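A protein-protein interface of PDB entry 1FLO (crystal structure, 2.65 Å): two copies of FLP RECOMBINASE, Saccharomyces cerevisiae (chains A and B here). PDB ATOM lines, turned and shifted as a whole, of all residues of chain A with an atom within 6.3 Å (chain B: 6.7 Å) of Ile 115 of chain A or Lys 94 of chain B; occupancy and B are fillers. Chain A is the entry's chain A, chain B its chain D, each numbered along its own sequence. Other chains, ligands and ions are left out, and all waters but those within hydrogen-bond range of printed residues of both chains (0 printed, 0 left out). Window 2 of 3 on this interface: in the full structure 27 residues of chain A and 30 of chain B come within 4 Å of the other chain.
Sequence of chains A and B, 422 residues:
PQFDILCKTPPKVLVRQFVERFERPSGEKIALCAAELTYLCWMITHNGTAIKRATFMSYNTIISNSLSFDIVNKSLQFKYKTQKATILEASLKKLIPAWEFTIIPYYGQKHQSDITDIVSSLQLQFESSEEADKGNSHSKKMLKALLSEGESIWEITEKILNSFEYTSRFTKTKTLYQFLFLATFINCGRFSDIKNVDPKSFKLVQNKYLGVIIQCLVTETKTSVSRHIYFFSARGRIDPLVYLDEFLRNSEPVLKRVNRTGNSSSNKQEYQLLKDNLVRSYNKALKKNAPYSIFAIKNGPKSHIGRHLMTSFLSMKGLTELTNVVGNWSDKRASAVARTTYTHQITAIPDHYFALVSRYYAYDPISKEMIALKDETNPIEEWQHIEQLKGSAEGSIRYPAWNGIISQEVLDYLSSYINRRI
Among the printed residues, pairs that only touch across the chains: Ile 115 of chain A with Ser 91 of chain B, Ile 115 of chain A with Lys 94 of chain B, Ile 115 of chain A with Leu 95 of chain B and Val 119 of chain A with Val 15 of chain B.
Asp 114 of chain A touches none of the printed residues of chain B.
Ile 115 of chain A touches just these residues of chain B: Ser 91 (3.3 Å), Lys 94 (3.6 Å) and Leu 95 (3.4 Å).
Thr 116 of chain A touches none of the printed residues of chain B.
Of the printed residues of chain B, Val 119 of chain A touches Val 15.
Of the printed residues of chain A, Val 15 of chain B touches Val 119.
Printed residues of chain A within 4 Å of Ser 91 of chain B: Ile 115 (3.3 Å).
Of chain A, only Ile 115 (3.6 Å) comes within 4 Å of Lys 94 of chain B.
Printed residues of chain A within 4 Å of Leu 95 of chain B: Ile 115.
Hydrophobic or aromatic side chains of chain B within 4 Å of the printed part of chain A: Val 15 and Leu 95.
No position is printed for both chains.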
ATOM      1  N   SER A 113      27.582  17.005 -37.137  1.00  0.00           N
ATOM      2  CA  SER A 113      26.956  17.531 -35.928  1.00  0.00           C
ATOM      3  C   SER A 113      27.020  16.531 -34.773  1.00  0.00           C
ATOM      4  O   SER A 113      25.981  16.061 -34.290  1.00  0.00           O
ATOM      5  CB  SER A 113      25.488  17.901 -36.199  1.00  0.00           C
ATOM      6  OG  SER A 113      25.370  18.900 -37.197  1.00  0.00           O
ATOM      7  N   ASP A 114      28.229  16.187 -34.337  1.00  0.00           N
ATOM      8  CA  ASP A 114      28.346  15.266 -33.217  1.00  0.00           C
ATOM      9  C   ASP A 114      27.939  16.013 -31.958  1.00  0.00           C
ATOM     10  O   ASP A 114      28.350  17.157 -31.747  1.00  0.00           O
ATOM     11  CB  ASP A 114      29.771  14.758 -33.039  1.00  0.00           C
ATOM     12  CG  ASP A 114      29.976  14.107 -31.682  1.00  0.00           C
ATOM     13  OD1 ASP A 114      29.280  13.107 -31.389  1.00  0.00           O
ATOM     14  OD2 ASP A 114      30.821  14.601 -30.906  1.00  0.00           O
ATOM     15  N   ILE A 115      27.133  15.362 -31.126  1.00  0.00           N
ATOM     16  CA  ILE A 115      26.666  15.970 -29.889  1.00  0.00           C
ATOM     17  C   ILE A 115      27.816  16.427 -28.981  1.00  0.00           C
ATOM     18  O   ILE A 115      27.714  17.460 -28.314  1.00  0.00           O
ATOM     19  CB  ILE A 115      25.767  14.988 -29.125  1.00  0.00           C
ATOM     20  CG1 ILE A 115      26.524  13.681 -28.862  1.00  0.00           C
ATOM     21  CG2 ILE A 115      24.511  14.713 -29.939  1.00  0.00           C
ATOM     22  CD1 ILE A 115      25.755  12.666 -28.027  1.00  0.00           C
ATOM     23  N   THR A 116      28.910  15.669 -28.969  1.00  0.00           N
ATOM     24  CA  THR A 116      30.066  16.006 -28.139  1.00  0.00           C
ATOM     25  C   THR A 116      30.924  17.112 -28.761  1.00  0.00           C
ATOM     26  O   THR A 116      31.412  17.990 -28.052  1.00  0.00           O
ATOM     27  CB  THR A 116      30.940  14.758 -27.876  1.00  0.00           C
ATOM     28  OG1 THR A 116      30.179  13.784 -27.149  1.00  0.00           O
ATOM     29  CG2 THR A 116      32.168  15.123 -27.066  1.00  0.00           C
ATOM     30  N   ASP A 117      31.117  17.063 -30.077  1.00  0.00           N
ATOM     31  CA  ASP A 117      31.897  18.089 -30.775  1.00  0.00           C
ATOM     32  C   ASP A 117      31.187  19.422 -30.524  1.00  0.00           C
ATOM     33  O   ASP A 117      31.793  20.498 -30.512  1.00  0.00           O
ATOM     34  CB  ASP A 117      31.939  17.799 -32.285  1.00  0.00           C
ATOM     35  CG  ASP A 117      33.029  16.801 -32.669  1.00  0.00           C
ATOM     36  OD1 ASP A 117      34.214  17.198 -32.738  1.00  0.00           O
ATOM     37  OD2 ASP A 117      32.702  15.618 -32.903  1.00  0.00           O
ATOM     38  N   ILE A 118      29.881  19.318 -30.321  1.00  0.00           N
ATOM     39  CA  ILE A 118      29.034  20.464 -30.049  1.00  0.00           C
ATOM     40  C   ILE A 118      29.176  20.859 -28.572  1.00  0.00           C
ATOM     41  O   ILE A 118      29.399  22.031 -28.258  1.00  0.00           O
ATOM     42  CB  ILE A 118      27.569  20.116 -30.394  1.00  0.00           C
ATOM     43  CG1 ILE A 118      27.439  19.944 -31.915  1.00  0.00           C
ATOM     44  CG2 ILE A 118      26.634  21.176 -29.856  1.00  0.00           C
ATOM     45  CD1 ILE A 118      26.058  19.537 -32.390  1.00  0.00           C
ATOM     46  N   VAL A 119      29.065  19.883 -27.672  1.00  0.00           N
ATOM     47  CA  VAL A 119      29.203  20.147 -26.238  1.00  0.00           C
ATOM     48  C   VAL A 119      30.578  20.738 -25.934  1.00  0.00           C
ATOM     49  O   VAL A 119      30.719  21.606 -25.065  1.00  0.00           O
ATOM     50  CB  VAL A 119      29.053  18.860 -25.394  1.00  0.00           C
ATOM     51  CG1 VAL A 119      29.278  19.184 -23.911  1.00  0.00           C
ATOM     52  CG2 VAL A 119      27.681  18.245 -25.611  1.00  0.00           C
ATOM     53  N   SER A 120      31.592  20.248 -26.645  1.00  0.00           N
ATOM     54  CA  SER A 120      32.956  20.726 -26.460  1.00  0.00           C
ATOM     55  C   SER A 120      32.997  22.203 -26.820  1.00  0.00           C
ATOM     56  O   SER A 120      33.299  23.050 -25.978  1.00  0.00           O
ATOM     57  CB  SER A 120      33.932  19.941 -27.353  1.00  0.00           C
ATOM     58  OG  SER A 120      33.741  20.231 -28.732  1.00  0.00           O
ATOM     59  N   VAL B  15      25.936  17.766 -19.605  1.00  0.00           N
ATOM     60  CA  VAL B  15      25.961  16.494 -20.329  1.00  0.00           C
ATOM     61  C   VAL B  15      26.283  15.386 -19.344  1.00  0.00           C
ATOM     62  O   VAL B  15      25.967  14.218 -19.570  1.00  0.00           O
ATOM     63  CB  VAL B  15      27.044  16.474 -21.434  1.00  0.00           C
ATOM     64  CG1 VAL B  15      26.847  17.655 -22.370  1.00  0.00           C
ATOM     65  CG2 VAL B  15      28.441  16.493 -20.812  1.00  0.00           C
ATOM     66  N   ILE B  44      21.288  20.299 -30.099  1.00  0.00           N
ATOM     67  CA  ILE B  44      21.468  19.148 -30.976  1.00  0.00           C
ATOM     68  C   ILE B  44      20.987  19.450 -32.389  1.00  0.00           C
ATOM     69  O   ILE B  44      21.744  19.325 -33.356  1.00  0.00           O
ATOM     70  CB  ILE B  44      20.691  17.914 -30.446  1.00  0.00           C
ATOM     71  CG1 ILE B  44      21.242  17.487 -29.085  1.00  0.00           C
ATOM     72  CG2 ILE B  44      20.799  16.768 -31.438  1.00  0.00           C
ATOM     73  CD1 ILE B  44      20.478  16.354 -28.442  1.00  0.00           C
ATOM     74  N   ILE B  87      17.375  12.255 -36.593  1.00  0.00           N
ATOM     75  CA  ILE B  87      18.713  12.587 -36.126  1.00  0.00           C
ATOM     76  C   ILE B  87      18.791  12.813 -34.618  1.00  0.00           C
ATOM     77  O   ILE B  87      19.744  12.366 -33.980  1.00  0.00           O
ATOM     78  CB  ILE B  87      19.256  13.834 -36.851  1.00  0.00           C
ATOM     79  CG1 ILE B  87      19.334  13.561 -38.360  1.00  0.00           C
ATOM     80  CG2 ILE B  87      20.627  14.201 -36.294  1.00  0.00           C
ATOM     81  CD1 ILE B  87      19.781  14.756 -39.195  1.00  0.00           C
ATOM     82  N   GLU B  89      17.242  11.426 -32.501  1.00  0.00           N
ATOM     83  CA  GLU B  89      17.178  10.102 -31.897  1.00  0.00           C
ATOM     84  C   GLU B  89      18.617   9.569 -31.853  1.00  0.00           C
ATOM     85  O   GLU B  89      19.135   9.234 -30.783  1.00  0.00           O
ATOM     86  CB  GLU B  89      16.306   9.160 -32.745  1.00  0.00           C
ATOM     87  CG  GLU B  89      14.873   9.631 -32.998  1.00  0.00           C
ATOM     88  CD  GLU B  89      14.001   9.602 -31.760  1.00  0.00           C
ATOM     89  OE1 GLU B  89      14.472  10.058 -30.695  1.00  0.00           O
ATOM     90  OE2 GLU B  89      12.842   9.133 -31.861  1.00  0.00           O
ATOM     91  N   ALA B  90      19.251   9.513 -33.029  1.00  0.00           N
ATOM     92  CA  ALA B  90      20.628   9.026 -33.181  1.00  0.00           C
ATOM     93  C   ALA B  90      21.597   9.741 -32.242  1.00  0.00           C
ATOM     94  O   ALA B  90      22.571   9.147 -31.761  1.00  0.00           O
ATOM     95  CB  ALA B  90      21.085   9.196 -34.634  1.00  0.00           C
ATOM     96  N   SER B  91      21.332  11.020 -31.994  1.00  0.00           N
ATOM     97  CA  SER B  91      22.171  11.805 -31.102  1.00  0.00           C
ATOM     98  C   SER B  91      21.890  11.415 -29.658  1.00  0.00           C
ATOM     99  O   SER B  91      22.805  11.042 -28.931  1.00  0.00           O
ATOM    100  CB  SER B  91      21.919  13.303 -31.304  1.00  0.00           C
ATOM    101  OG  SER B  91      22.569  13.779 -32.472  1.00  0.00           O
ATOM    102  N   LEU B  92      20.625  11.492 -29.249  1.00  0.00           N
ATOM    103  CA  LEU B  92      20.230  11.136 -27.884  1.00  0.00           C
ATOM    104  C   LEU B  92      20.696   9.728 -27.508  1.00  0.00           C
ATOM    105  O   LEU B  92      21.022   9.459 -26.345  1.00  0.00           O
ATOM    106  CB  LEU B  92      18.707  11.222 -27.730  1.00  0.00           C
ATOM    107  CG  LEU B  92      18.062  12.608 -27.693  1.00  0.00           C
ATOM    108  CD1 LEU B  92      16.546  12.454 -27.758  1.00  0.00           C
ATOM    109  CD2 LEU B  92      18.488  13.349 -26.424  1.00  0.00           C
ATOM    110  N   LYS B  93      20.713   8.835 -28.497  1.00  0.00           N
ATOM    111  CA  LYS B  93      21.146   7.452 -28.301  1.00  0.00           C
ATOM    112  C   LYS B  93      22.616   7.417 -27.864  1.00  0.00           C
ATOM    113  O   LYS B  93      22.948   6.827 -26.833  1.00  0.00           O
ATOM    114  CB  LYS B  93      20.978   6.662 -29.605  1.00  0.00           C
ATOM    115  CG  LYS B  93      21.391   5.196 -29.534  1.00  0.00           C
ATOM    116  CD  LYS B  93      20.381   4.349 -28.774  1.00  0.00           C
ATOM    117  CE  LYS B  93      20.782   2.880 -28.805  1.00  0.00           C
ATOM    118  NZ  LYS B  93      19.788   2.004 -28.126  1.00  0.00           N
ATOM    119  N   LYS B  94      23.489   8.057 -28.644  1.00  0.00           N
ATOM    120  CA  LYS B  94      24.915   8.094 -28.328  1.00  0.00           C
ATOM    121  C   LYS B  94      25.267   8.835 -27.034  1.00  0.00           C
ATOM    122  O   LYS B  94      26.378   9.348 -26.887  1.00  0.00           O
ATOM    123  CB  LYS B  94      25.697   8.707 -29.487  1.00  0.00           C
ATOM    124  CG  LYS B  94      26.022   7.727 -30.592  1.00  0.00           C
ATOM    125  CD  LYS B  94      27.160   8.262 -31.439  1.00  0.00           C
ATOM    126  CE  LYS B  94      27.669   7.213 -32.410  1.00  0.00           C
ATOM    127  NZ  LYS B  94      28.804   7.726 -33.234  1.00  0.00           N
ATOM    128  N   LEU B  95      24.315   8.892 -26.107  1.00  0.00           N
ATOM    129  CA  LEU B  95      24.509   9.538 -24.807  1.00  0.00           C
ATOM    130  C   LEU B  95      24.285   8.481 -23.726  1.00  0.00           C
ATOM    131  O   LEU B  95      25.154   8.235 -22.888  1.00  0.00           O
ATOM    132  CB  LEU B  95      23.525  10.704 -24.623  1.00  0.00           C
ATOM    133  CG  LEU B  95      23.929  12.054 -25.227  1.00  0.00           C
ATOM    134  CD1 LEU B  95      22.785  13.060 -25.096  1.00  0.00           C
ATOM    135  CD2 LEU B  95      25.175  12.566 -24.515  1.00  0.00           C
ATOM    136  N   ILE B  96      23.111   7.861 -23.757  1.00  0.00           N
ATOM    137  CA  ILE B  96      22.770   6.802 -22.816  1.00  0.00           C
ATOM    138  C   ILE B  96      22.302   5.631 -23.685  1.00  0.00           C
ATOM    139  O   ILE B  96      21.142   5.213 -23.604  1.00  0.00           O
ATOM    140  CB  ILE B  96      21.623   7.226 -21.854  1.00  0.00           C
ATOM    141  CG1 ILE B  96      22.041   8.429 -20.998  1.00  0.00           C
ATOM    142  CG2 ILE B  96      21.275   6.076 -20.929  1.00  0.00           C
ATOM    143  CD1 ILE B  96      22.028   9.767 -21.717  1.00  0.00           C
ATOM    144  N   PRO B  97      23.204   5.088 -24.534  1.00  0.00           N
ATOM    145  CA  PRO B  97      22.918   3.968 -25.444  1.00  0.00           C
ATOM    146  C   PRO B  97      22.063   2.824 -24.890  1.00  0.00           C
ATOM    147  O   PRO B  97      21.469   2.059 -25.654  1.00  0.00           O
ATOM    148  CB  PRO B  97      24.315   3.506 -25.864  1.00  0.00           C
ATOM    149  CG  PRO B  97      25.074   4.797 -25.916  1.00  0.00           C
ATOM    150  CD  PRO B  97      24.631   5.466 -24.622  1.00  0.00           C
ATOM    151  N   PHE B 101      14.919   6.189 -26.976  1.00  0.00           N
ATOM    152  CA  PHE B 101      14.065   7.376 -26.894  1.00  0.00           C
ATOM    153  C   PHE B 101      13.123   7.489 -28.087  1.00  0.00           C
ATOM    154  O   PHE B 101      13.329   6.851 -29.124  1.00  0.00           O
ATOM    155  CB  PHE B 101      14.911   8.653 -26.819  1.00  0.00           C
ATOM    156  CG  PHE B 101      16.109   8.545 -25.917  1.00  0.00           C
ATOM    157  CD1 PHE B 101      17.296   7.969 -26.378  1.00  0.00           C
ATOM    158  CD2 PHE B 101      16.055   9.022 -24.606  1.00  0.00           C
ATOM    159  CE1 PHE B 101      18.416   7.869 -25.546  1.00  0.00           C
ATOM    160  CE2 PHE B 101      17.169   8.930 -23.760  1.00  0.00           C
ATOM    161  CZ  PHE B 101      18.352   8.353 -24.231  1.00  0.00           C
